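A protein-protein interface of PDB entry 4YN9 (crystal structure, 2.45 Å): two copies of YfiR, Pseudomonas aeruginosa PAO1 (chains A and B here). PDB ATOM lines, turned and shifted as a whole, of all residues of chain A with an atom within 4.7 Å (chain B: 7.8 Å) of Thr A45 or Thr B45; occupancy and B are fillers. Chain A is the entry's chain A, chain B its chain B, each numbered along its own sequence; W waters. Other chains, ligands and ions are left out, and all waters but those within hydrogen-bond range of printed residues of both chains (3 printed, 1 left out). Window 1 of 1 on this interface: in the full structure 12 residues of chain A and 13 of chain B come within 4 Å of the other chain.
Printed residues of chain B that touch a printed residue of chain A: Ile B10, Gly B43, Pro B44, Thr B45, Glu B46, Asp B49, Arg B67 and Arg B110. Along chain B the printed residues that touch a printed residue of chain A span positions 10 to 110. Hydrophobic or aromatic side chains of chain A within 4 Å of the printed part of chain B: Pro A44. Among the printed residues, Asp or Glu carboxylates within 4 Å of a Lys or Arg side-chain nitrogen of the other chain: Arg A67 with Asp B49.
N of Glu A46 lies within hydrogen-bond range of OE2 of Glu A109 (2.7 Å). The backbone NH of Val B86 is in hydrogen-bond range of the backbone carbonyl oxygen of Pro B44, at 3.0 Å. The guanidinium group (NH1) of Arg B67 sits at hydrogen-bond distance from the side-chain hydroxyl (OG1) of Thr B45, at 3.2 Å. N of Glu B46 lies within hydrogen-bond range of OE2 of Glu B109, at 2.8 Å. The side-chain carboxylate (OE2) of Glu B46 is in salt-bridge range of the guanidinium group (NH2) of Arg B110 (3.4 Å). O of Arg B110 sits at hydrogen-bond distance from OG of Ser B108 (2.8 Å).
The backbone carbonyl oxygen of Thr B45 is in hydrogen-bond range of the backbone NH of Thr A45. The backbone carbonyl oxygen (O) of Thr A45 is in hydrogen-bond range of the guanidinium group (NH1) of Arg B67, at 3.4 Å. The backbone carbonyl oxygen (O) of Glu A46 lies close to the guanidinium group (NE) of Arg B67 (3.5 Å). The guanidinium group (NH2) of Arg A67 sits at hydrogen-bond distance from the backbone carbonyl oxygen (O) of Thr B45 (3.1 Å). The backbone carbonyl oxygen of Glu B46 sits at hydrogen-bond distance from the guanidinium group of Arg A67, 3.4 Å away. OD1 of Asp B49 lies within salt-bridge range of NH1 of Arg A67, at 2.9 Å.
Thr A45 touches just these residues of chain B: Pro B44, Thr B45 and Arg B67. Of chain A, only Pro A44 (3.4 Å), Thr A45 (3.1 Å) and Arg A67 (3.1 Å) come within 4 Å of Thr B45. Printed residues of chain B within 4 Å of Arg A67: Ile B10 (3.7 Å), Thr B45 (3.1 Å), Glu B46 (3.4 Å) and Asp B49 (2.9 Å). Printed residues of chain A within 4 Å of Arg B67: Thr A45 (3.4 Å) and Glu A46 (3.3 Å). Of the printed residues of chain A, Arg B110 touches Pro A44 (3.4 Å). Printed residues of chain A within 4 Å of Pro B44: Pro A44 (3.5 Å), Thr A45 (3.6 Å) and Glu A46 (3.4 Å). Tyr B47 touches none of the printed residues of chain A. Ile B107 touches none of the printed residues of chain A.
Glu B46 touches Gly A43 (CG to C, 3.4 Å). CB of Pro A44 touches O of Pro B44, 3.5 Å away. Pro A44 touches Thr B45 (CA to O, 3.4 Å). Pro A44 touches Glu B46 (N to CG, 3.5 Å). CG of Pro A44 touches NH2 of Arg B110, at 3.4 Å. Pro B44 touches Thr A45 (CA to C, 3.6 Å). Glu A46 touches Gly B43 (CG to C, 3.5 Å). Glu A46 touches Pro B44 (CG to N, 3.4 Å). Ile B10 touches Arg A67.
Water W2 bridges the side-chain carboxylate of Glu B46 and the backbone NH of Gly A43. Water W3 lies within hydrogen-bond range of OE1 of Glu A46 (2.7 Å) and N of Gly B43 (2.9 Å). Water W1 lies within hydrogen-bond range of O of Thr A45, N of Ala A48, NH2 of Arg B67 and O of Glu A46.
Pro B44 touches its own counterpart, Pro A44. Pro A44 touches Thr B45, and with the chains exchanged Thr A45 touches Pro B44. Thr B45 touches its own counterpart, Thr A45. Thr A45 touches Arg B67, and with the chains exchanged Arg A67 touches Thr B45.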
ATOM      1  N   VAL A  41     -28.290  22.104  -7.617  1.00  0.00           N
ATOM      2  CA  VAL A  41     -27.142  21.473  -8.249  1.00  0.00           C
ATOM      3  C   VAL A  41     -27.510  21.157  -9.696  1.00  0.00           C
ATOM      4  O   VAL A  41     -28.500  20.477  -9.962  1.00  0.00           O
ATOM      5  CB  VAL A  41     -26.718  20.167  -7.526  1.00  0.00           C
ATOM      6  CG1 VAL A  41     -25.663  19.424  -8.334  1.00  0.00           C
ATOM      7  CG2 VAL A  41     -26.232  20.458  -6.118  1.00  0.00           C
ATOM      8  N   GLY A  43     -26.263  19.870 -13.510  1.00  0.00           N
ATOM      9  CA  GLY A  43     -25.305  19.173 -14.352  1.00  0.00           C
ATOM     10  C   GLY A  43     -24.551  18.120 -13.565  1.00  0.00           C
ATOM     11  O   GLY A  43     -24.700  18.035 -12.351  1.00  0.00           O
ATOM     12  N   PRO A  44     -23.736  17.308 -14.255  1.00  0.00           N
ATOM     13  CA  PRO A  44     -22.998  16.221 -13.601  1.00  0.00           C
ATOM     14  C   PRO A  44     -21.951  16.737 -12.625  1.00  0.00           C
ATOM     15  O   PRO A  44     -21.162  17.608 -12.980  1.00  0.00           O
ATOM     16  CB  PRO A  44     -22.326  15.481 -14.766  1.00  0.00           C
ATOM     17  CG  PRO A  44     -23.053  15.916 -15.991  1.00  0.00           C
ATOM     18  CD  PRO A  44     -23.535  17.315 -15.714  1.00  0.00           C
ATOM     19  N   THR A  45     -21.942  16.194 -11.415  1.00  0.00           N
ATOM     20  CA  THR A  45     -21.000  16.629 -10.388  1.00  0.00           C
ATOM     21  C   THR A  45     -20.350  15.439  -9.693  1.00  0.00           C
ATOM     22  O   THR A  45     -20.970  14.382  -9.544  1.00  0.00           O
ATOM     23  CB  THR A  45     -21.680  17.486  -9.309  1.00  0.00           C
ATOM     24  OG1 THR A  45     -22.803  16.775  -8.790  1.00  0.00           O
ATOM     25  CG2 THR A  45     -22.146  18.815  -9.858  1.00  0.00           C
ATOM     26  N   GLU A  46     -19.104  15.624  -9.264  1.00  0.00           N
ATOM     27  CA  GLU A  46     -18.396  14.624  -8.473  1.00  0.00           C
ATOM     28  C   GLU A  46     -18.562  14.874  -6.984  1.00  0.00           C
ATOM     29  O   GLU A  46     -18.626  13.938  -6.194  1.00  0.00           O
ATOM     30  CB  GLU A  46     -16.903  14.624  -8.788  1.00  0.00           C
ATOM     31  CG  GLU A  46     -16.499  13.780  -9.937  1.00  0.00           C
ATOM     32  CD  GLU A  46     -15.002  13.770 -10.131  1.00  0.00           C
ATOM     33  OE1 GLU A  46     -14.377  12.770  -9.715  1.00  0.00           O
ATOM     34  OE2 GLU A  46     -14.461  14.754 -10.697  1.00  0.00           O
ATOM     35  N   TYR A  47     -18.614  16.147  -6.611  1.00  0.00           N
ATOM     36  CA  TYR A  47     -18.380  16.533  -5.224  1.00  0.00           C
ATOM     37  C   TYR A  47     -19.566  17.165  -4.528  1.00  0.00           C
ATOM     38  O   TYR A  47     -19.387  17.883  -3.543  1.00  0.00           O
ATOM     39  CB  TYR A  47     -17.201  17.500  -5.166  1.00  0.00           C
ATOM     40  CG  TYR A  47     -15.956  16.911  -5.757  1.00  0.00           C
ATOM     41  CD1 TYR A  47     -15.268  15.891  -5.091  1.00  0.00           C
ATOM     42  CD2 TYR A  47     -15.464  17.355  -6.976  1.00  0.00           C
ATOM     43  CE1 TYR A  47     -14.111  15.336  -5.618  1.00  0.00           C
ATOM     44  CE2 TYR A  47     -14.315  16.804  -7.520  1.00  0.00           C
ATOM     45  CZ  TYR A  47     -13.640  15.793  -6.828  1.00  0.00           C
ATOM     46  OH  TYR A  47     -12.493  15.246  -7.347  1.00  0.00           O
ATOM     47  N   ALA A  48     -20.768  16.898  -5.024  1.00  0.00           N
ATOM     48  CA  ALA A  48     -21.954  17.572  -4.507  1.00  0.00           C
ATOM     49  C   ALA A  48     -22.735  16.721  -3.510  1.00  0.00           C
ATOM     50  O   ALA A  48     -23.738  17.173  -2.968  1.00  0.00           O
ATOM     51  CB  ALA A  48     -22.848  17.974  -5.653  1.00  0.00           C
ATOM     52  N   ARG A  67     -30.990  18.519  -7.036  1.00  0.00           N
ATOM     53  CA  ARG A  67     -30.536  18.571  -8.415  1.00  0.00           C
ATOM     54  C   ARG A  67     -31.646  19.108  -9.281  1.00  0.00           C
ATOM     55  O   ARG A  67     -32.818  18.904  -8.973  1.00  0.00           O
ATOM     56  CB  ARG A  67     -30.108  17.183  -8.926  1.00  0.00           C
ATOM     57  CG  ARG A  67     -29.369  16.351  -7.926  1.00  0.00           C
ATOM     58  CD  ARG A  67     -28.643  15.181  -8.606  1.00  0.00           C
ATOM     59  NE  ARG A  67     -27.406  15.646  -9.206  1.00  0.00           N
ATOM     60  CZ  ARG A  67     -26.191  15.355  -8.767  1.00  0.00           C
ATOM     61  NH1 ARG A  67     -26.018  14.552  -7.723  1.00  0.00           N
ATOM     62  NH2 ARG A  67     -25.141  15.859  -9.403  1.00  0.00           N
ATOM     63  N   TYR A  83     -24.972  25.444  -7.866  1.00  0.00           N
ATOM     64  CA  TYR A  83     -23.685  24.763  -7.904  1.00  0.00           C
ATOM     65  C   TYR A  83     -23.641  24.067  -9.265  1.00  0.00           C
ATOM     66  O   TYR A  83     -24.407  23.127  -9.538  1.00  0.00           O
ATOM     67  CB  TYR A  83     -23.529  23.784  -6.723  1.00  0.00           C
ATOM     68  CG  TYR A  83     -22.227  23.012  -6.676  1.00  0.00           C
ATOM     69  CD1 TYR A  83     -21.114  23.507  -5.999  1.00  0.00           C
ATOM     70  CD2 TYR A  83     -22.115  21.774  -7.301  1.00  0.00           C
ATOM     71  CE1 TYR A  83     -19.922  22.799  -5.965  1.00  0.00           C
ATOM     72  CE2 TYR A  83     -20.945  21.059  -7.273  1.00  0.00           C
ATOM     73  CZ  TYR A  83     -19.851  21.563  -6.605  1.00  0.00           C
ATOM     74  OH  TYR A  83     -18.696  20.811  -6.598  1.00  0.00           O
ATOM     75  N   GLY A  85     -22.152  22.032 -12.434  1.00  0.00           N
ATOM     76  CA  GLY A  85     -21.237  20.971 -12.809  1.00  0.00           C
ATOM     77  C   GLY A  85     -20.854  21.097 -14.272  1.00  0.00           C
ATOM     78  O   GLY A  85     -20.827  22.197 -14.819  1.00  0.00           O
ATOM     79  N   GLU A 109     -18.058  23.653  -9.836  1.00  0.00           N
ATOM     80  CA  GLU A 109     -17.236  22.589  -9.306  1.00  0.00           C
ATOM     81  C   GLU A 109     -15.839  22.638  -9.906  1.00  0.00           C
ATOM     82  O   GLU A 109     -14.859  22.281  -9.242  1.00  0.00           O
ATOM     83  CB  GLU A 109     -17.887  21.236  -9.596  1.00  0.00           C
ATOM     84  CG  GLU A 109     -17.016  20.036  -9.269  1.00  0.00           C
ATOM     85  CD  GLU A 109     -17.833  18.782  -9.111  1.00  0.00           C
ATOM     86  OE1 GLU A 109     -18.544  18.685  -8.086  1.00  0.00           O
ATOM     87  OE2 GLU A 109     -17.775  17.909 -10.007  1.00  0.00           O
ATOM     88  N   ILE B  10     -35.071  15.198 -12.451  1.00  0.00           N
ATOM     89  CA  ILE B  10     -33.749  14.607 -12.242  1.00  0.00           C
ATOM     90  C   ILE B  10     -33.850  13.489 -11.219  1.00  0.00           C
ATOM     91  O   ILE B  10     -33.238  12.435 -11.391  1.00  0.00           O
ATOM     92  CB  ILE B  10     -32.697  15.632 -11.765  1.00  0.00           C
ATOM     93  CG1 ILE B  10     -32.483  16.706 -12.824  1.00  0.00           C
ATOM     94  CG2 ILE B  10     -31.374  14.938 -11.533  1.00  0.00           C
ATOM     95  CD1 ILE B  10     -31.723  16.205 -14.018  1.00  0.00           C
ATOM     96  N   VAL B  41     -19.042   4.460  -8.546  1.00  0.00           N
ATOM     97  CA  VAL B  41     -19.397   5.607  -9.361  1.00  0.00           C
ATOM     98  C   VAL B  41     -18.174   6.494  -9.589  1.00  0.00           C
ATOM     99  O   VAL B  41     -17.509   6.903  -8.640  1.00  0.00           O
ATOM    100  CB  VAL B  41     -20.501   6.435  -8.716  1.00  0.00           C
ATOM    101  CG1 VAL B  41     -20.791   7.652  -9.578  1.00  0.00           C
ATOM    102  CG2 VAL B  41     -21.744   5.588  -8.527  1.00  0.00           C
ATOM    103  N   VAL B  42     -17.883   6.781 -10.853  1.00  0.00           N
ATOM    104  CA  VAL B  42     -16.603   7.349 -11.239  1.00  0.00           C
ATOM    105  C   VAL B  42     -16.779   8.493 -12.232  1.00  0.00           C
ATOM    106  O   VAL B  42     -17.272   8.298 -13.351  1.00  0.00           O
ATOM    107  CB  VAL B  42     -15.675   6.264 -11.859  1.00  0.00           C
ATOM    108  CG1 VAL B  42     -14.381   6.884 -12.356  1.00  0.00           C
ATOM    109  CG2 VAL B  42     -15.386   5.141 -10.847  1.00  0.00           C
ATOM    110  N   GLY B  43     -16.365   9.686 -11.821  1.00  0.00           N
ATOM    111  CA  GLY B  43     -16.564  10.871 -12.628  1.00  0.00           C
ATOM    112  C   GLY B  43     -17.847  11.610 -12.268  1.00  0.00           C
ATOM    113  O   GLY B  43     -18.689  11.118 -11.508  1.00  0.00           O
ATOM    114  N   PRO B  44     -18.003  12.816 -12.803  1.00  0.00           N
ATOM    115  CA  PRO B  44     -19.194  13.638 -12.589  1.00  0.00           C
ATOM    116  C   PRO B  44     -20.444  12.972 -13.139  1.00  0.00           C
ATOM    117  O   PRO B  44     -20.435  12.553 -14.286  1.00  0.00           O
ATOM    118  CB  PRO B  44     -18.876  14.918 -13.371  1.00  0.00           C
ATOM    119  CG  PRO B  44     -17.394  14.973 -13.389  1.00  0.00           C
ATOM    120  CD  PRO B  44     -16.950  13.546 -13.525  1.00  0.00           C
ATOM    121  N   THR B  45     -21.504  12.903 -12.345  1.00  0.00           N
ATOM    122  CA  THR B  45     -22.751  12.270 -12.769  1.00  0.00           C
ATOM    123  C   THR B  45     -23.968  13.088 -12.373  1.00  0.00           C
ATOM    124  O   THR B  45     -23.947  13.795 -11.363  1.00  0.00           O
ATOM    125  CB  THR B  45     -22.904  10.867 -12.163  1.00  0.00           C
ATOM    126  OG1 THR B  45     -22.794  10.943 -10.726  1.00  0.00           O
ATOM    127  CG2 THR B  45     -21.832   9.940 -12.708  1.00  0.00           C
ATOM    128  N   GLU B  46     -25.032  12.992 -13.167  1.00  0.00           N
ATOM    129  CA  GLU B  46     -26.291  13.647 -12.829  1.00  0.00           C
ATOM    130  C   GLU B  46     -27.264  12.689 -12.178  1.00  0.00           C
ATOM    131  O   GLU B  46     -28.125  13.085 -11.401  1.00  0.00           O
ATOM    132  CB  GLU B  46     -26.957  14.203 -14.067  1.00  0.00           C
ATOM    133  CG  GLU B  46     -26.791  15.648 -14.320  1.00  0.00           C
ATOM    134  CD  GLU B  46     -27.476  16.054 -15.603  1.00  0.00           C
ATOM    135  OE1 GLU B  46     -28.277  17.005 -15.558  1.00  0.00           O
ATOM    136  OE2 GLU B  46     -27.219  15.410 -16.651  1.00  0.00           O
ATOM    137  N   TYR B  47     -27.162  11.417 -12.534  1.00  0.00           N
ATOM    138  CA  TYR B  47     -28.265  10.521 -12.245  1.00  0.00           C
ATOM    139  C   TYR B  47     -27.857   9.374 -11.344  1.00  0.00           C
ATOM    140  O   TYR B  47     -28.535   8.348 -11.303  1.00  0.00           O
ATOM    141  CB  TYR B  47     -28.861   9.990 -13.557  1.00  0.00           C
ATOM    142  CG  TYR B  47     -29.391  11.062 -14.503  1.00  0.00           C
ATOM    143  CD1 TYR B  47     -30.553  11.772 -14.213  1.00  0.00           C
ATOM    144  CD2 TYR B  47     -28.737  11.345 -15.698  1.00  0.00           C
ATOM    145  CE1 TYR B  47     -31.046  12.751 -15.093  1.00  0.00           C
ATOM    146  CE2 TYR B  47     -29.215  12.308 -16.581  1.00  0.00           C
ATOM    147  CZ  TYR B  47     -30.370  13.017 -16.277  1.00  0.00           C
ATOM    148  OH  TYR B  47     -30.834  13.987 -17.164  1.00  0.00           O
ATOM    149  N   ALA B  48     -26.769   9.542 -10.596  1.00  0.00           N
ATOM    150  CA  ALA B  48     -26.307   8.444  -9.755  1.00  0.00           C
ATOM    151  C   ALA B  48     -26.706   8.550  -8.274  1.00  0.00           C
ATOM    152  O   ALA B  48     -26.262   7.735  -7.467  1.00  0.00           O
ATOM    153  CB  ALA B  48     -24.790   8.300  -9.875  1.00  0.00           C
ATOM    154  N   ASP B  49     -27.558   9.503  -7.904  1.00  0.00           N
ATOM    155  CA  ASP B  49     -27.911   9.641  -6.482  1.00  0.00           C
ATOM    156  C   ASP B  49     -28.755   8.495  -5.904  1.00  0.00           C
ATOM    157  O   ASP B  49     -28.710   8.248  -4.703  1.00  0.00           O
ATOM    158  CB  ASP B  49     -28.636  10.956  -6.235  1.00  0.00           C
ATOM    159  CG  ASP B  49     -27.728  12.158  -6.397  1.00  0.00           C
ATOM    160  OD1 ASP B  49     -26.495  11.963  -6.565  1.00  0.00           O
ATOM    161  OD2 ASP B  49     -28.253  13.297  -6.362  1.00  0.00           O
ATOM    162  N   LEU B  51     -28.426   5.231  -7.062  1.00  0.00           N
ATOM    163  CA  LEU B  51     -27.444   4.167  -6.927  1.00  0.00           C
ATOM    164  C   LEU B  51     -26.696   4.332  -5.620  1.00  0.00           C
ATOM    165  O   LEU B  51     -26.463   3.367  -4.897  1.00  0.00           O
ATOM    166  CB  LEU B  51     -26.447   4.184  -8.078  1.00  0.00           C
ATOM    167  CG  LEU B  51     -27.013   4.146  -9.480  1.00  0.00           C
ATOM    168  CD1 LEU B  51     -25.867   4.283 -10.471  1.00  0.00           C
ATOM    169  CD2 LEU B  51     -27.756   2.834  -9.678  1.00  0.00           C
ATOM    170  N   LEU B  52     -26.319   5.574  -5.322  1.00  0.00           N
ATOM    171  CA  LEU B  52     -25.460   5.847  -4.180  1.00  0.00           C
ATOM    172  C   LEU B  52     -26.157   5.632  -2.830  1.00  0.00           C
ATOM    173  O   LEU B  52     -25.494   5.469  -1.817  1.00  0.00           O
ATOM    174  CB  LEU B  52     -24.896   7.268  -4.292  1.00  0.00           C
ATOM    175  CG  LEU B  52     -23.812   7.341  -5.379  1.00  0.00           C
ATOM    176  CD1 LEU B  52     -23.405   8.773  -5.687  1.00  0.00           C
ATOM    177  CD2 LEU B  52     -22.582   6.515  -4.992  1.00  0.00           C
ATOM    178  N   ARG B  67     -18.564   6.563  -4.434  1.00  0.00           N
ATOM    179  CA  ARG B  67     -17.783   7.245  -5.442  1.00  0.00           C
ATOM    180  C   ARG B  67     -16.321   6.921  -5.276  1.00  0.00           C
ATOM    181  O   ARG B  67     -15.820   6.760  -4.168  1.00  0.00           O
ATOM    182  CB  ARG B  67     -17.972   8.758  -5.374  1.00  0.00           C
ATOM    183  CG  ARG B  67     -19.292   9.214  -5.884  1.00  0.00           C
ATOM    184  CD  ARG B  67     -19.336  10.719  -5.967  1.00  0.00           C
ATOM    185  NE  ARG B  67     -20.693  11.168  -6.175  1.00  0.00           N
ATOM    186  CZ  ARG B  67     -21.229  11.371  -7.373  1.00  0.00           C
ATOM    187  NH1 ARG B  67     -20.499  11.166  -8.462  1.00  0.00           N
ATOM    188  NH2 ARG B  67     -22.487  11.788  -7.475  1.00  0.00           N
ATOM    189  N   TYR B  83     -20.002   2.609 -12.720  1.00  0.00           N
ATOM    190  CA  TYR B  83     -20.957   3.478 -13.368  1.00  0.00           C
ATOM    191  C   TYR B  83     -20.169   4.731 -13.700  1.00  0.00           C
ATOM    192  O   TYR B  83     -19.789   5.481 -12.804  1.00  0.00           O
ATOM    193  CB  TYR B  83     -22.157   3.758 -12.452  1.00  0.00           C
ATOM    194  CG  TYR B  83     -23.186   4.698 -13.033  1.00  0.00           C
ATOM    195  CD1 TYR B  83     -24.232   4.218 -13.813  1.00  0.00           C
ATOM    196  CD2 TYR B  83     -23.107   6.072 -12.812  1.00  0.00           C
ATOM    197  CE1 TYR B  83     -25.174   5.079 -14.357  1.00  0.00           C
ATOM    198  CE2 TYR B  83     -24.048   6.942 -13.347  1.00  0.00           C
ATOM    199  CZ  TYR B  83     -25.082   6.442 -14.113  1.00  0.00           C
ATOM    200  OH  TYR B  83     -26.024   7.303 -14.649  1.00  0.00           O
ATOM    201  N   LEU B  84     -19.908   4.926 -14.986  1.00  0.00           N
ATOM    202  CA  LEU B  84     -18.953   5.916 -15.476  1.00  0.00           C
ATOM    203  C   LEU B  84     -19.616   7.235 -15.914  1.00  0.00           C
ATOM    204  O   LEU B  84     -20.485   7.250 -16.787  1.00  0.00           O
ATOM    205  CB  LEU B  84     -18.165   5.315 -16.646  1.00  0.00           C
ATOM    206  CG  LEU B  84     -16.932   6.061 -17.153  1.00  0.00           C
ATOM    207  CD1 LEU B  84     -15.878   6.021 -16.075  1.00  0.00           C
ATOM    208  CD2 LEU B  84     -16.403   5.452 -18.455  1.00  0.00           C
ATOM    209  N   GLY B  85     -19.199   8.337 -15.305  1.00  0.00           N
ATOM    210  CA  GLY B  85     -19.726   9.649 -15.648  1.00  0.00           C
ATOM    211  C   GLY B  85     -18.834  10.322 -16.670  1.00  0.00           C
ATOM    212  O   GLY B  85     -18.152   9.650 -17.437  1.00  0.00           O
ATOM    213  N   VAL B  86     -18.842  11.652 -16.681  1.00  0.00           N
ATOM    214  CA  VAL B  86     -18.057  12.439 -17.630  1.00  0.00           C
ATOM    215  C   VAL B  86     -16.556  12.246 -17.439  1.00  0.00           C
ATOM    216  O   VAL B  86     -16.028  12.460 -16.354  1.00  0.00           O
ATOM    217  CB  VAL B  86     -18.383  13.944 -17.504  1.00  0.00           C
ATOM    218  CG1 VAL B  86     -17.430  14.783 -18.350  1.00  0.00           C
ATOM    219  CG2 VAL B  86     -19.825  14.208 -17.897  1.00  0.00           C
ATOM    220  N   ILE B 107     -20.840   0.582 -17.135  1.00  0.00           N
ATOM    221  CA  ILE B 107     -22.010   1.281 -17.644  1.00  0.00           C
ATOM    222  C   ILE B 107     -21.741   2.782 -17.608  1.00  0.00           C
ATOM    223  O   ILE B 107     -21.336   3.316 -16.576  1.00  0.00           O
ATOM    224  CB  ILE B 107     -23.273   0.950 -16.815  1.00  0.00           C
ATOM    225  CG1 ILE B 107     -23.504  -0.565 -16.798  1.00  0.00           C
ATOM    226  CG2 ILE B 107     -24.505   1.710 -17.350  1.00  0.00           C
ATOM    227  CD1 ILE B 107     -24.706  -1.007 -16.011  1.00  0.00           C
ATOM    228  N   SER B 108     -21.929   3.462 -18.734  1.00  0.00           N
ATOM    229  CA  SER B 108     -21.704   4.900 -18.772  1.00  0.00           C
ATOM    230  C   SER B 108     -23.030   5.662 -18.857  1.00  0.00           C
ATOM    231  O   SER B 108     -23.957   5.238 -19.523  1.00  0.00           O
ATOM    232  CB  SER B 108     -20.782   5.268 -19.932  1.00  0.00           C
ATOM    233  OG  SER B 108     -21.403   4.968 -21.152  1.00  0.00           O
ATOM    234  N   GLU B 109     -23.109   6.773 -18.138  1.00  0.00           N
ATOM    235  CA  GLU B 109     -24.331   7.559 -17.998  1.00  0.00           C
ATOM    236  C   GLU B 109     -24.726   8.245 -19.314  1.00  0.00           C
ATOM    237  O   GLU B 109     -25.913   8.425 -19.621  1.00  0.00           O
ATOM    238  CB  GLU B 109     -24.134   8.602 -16.877  1.00  0.00           C
ATOM    239  CG  GLU B 109     -25.250   9.592 -16.754  1.00  0.00           C
ATOM    240  CD  GLU B 109     -25.147  10.424 -15.511  1.00  0.00           C
ATOM    241  OE1 GLU B 109     -25.544   9.912 -14.444  1.00  0.00           O
ATOM    242  OE2 GLU B 109     -24.685  11.590 -15.600  1.00  0.00           O
ATOM    243  N   ARG B 110     -23.716   8.653 -20.075  1.00  0.00           N
ATOM    244  CA  ARG B 110     -23.919   9.194 -21.414  1.00  0.00           C
ATOM    245  C   ARG B 110     -23.316   8.235 -22.436  1.00  0.00           C
ATOM    246  O   ARG B 110     -22.553   7.335 -22.085  1.00  0.00           O
ATOM    247  CB  ARG B 110     -23.304  10.587 -21.516  1.00  0.00           C
ATOM    248  CG  ARG B 110     -23.898  11.522 -20.479  1.00  0.00           C
ATOM    249  CD  ARG B 110     -23.207  12.863 -20.393  1.00  0.00           C
ATOM    250  NE  ARG B 110     -24.027  13.785 -19.617  1.00  0.00           N
ATOM    251  CZ  ARG B 110     -23.935  15.107 -19.686  1.00  0.00           C
ATOM    252  NH1 ARG B 110     -23.038  15.660 -20.490  1.00  0.00           N
ATOM    253  NH2 ARG B 110     -24.740  15.872 -18.952  1.00  0.00           N
HETATM  254  O   HOH W   1     -21.829  14.773  -6.844  1.00  0.00           O
HETATM  255  O   HOH W   2     -28.460  18.271 -13.290  1.00  0.00           O
HETATM  256  O   HOH W   3     -15.504  10.356  -9.116  1.00  0.00           O
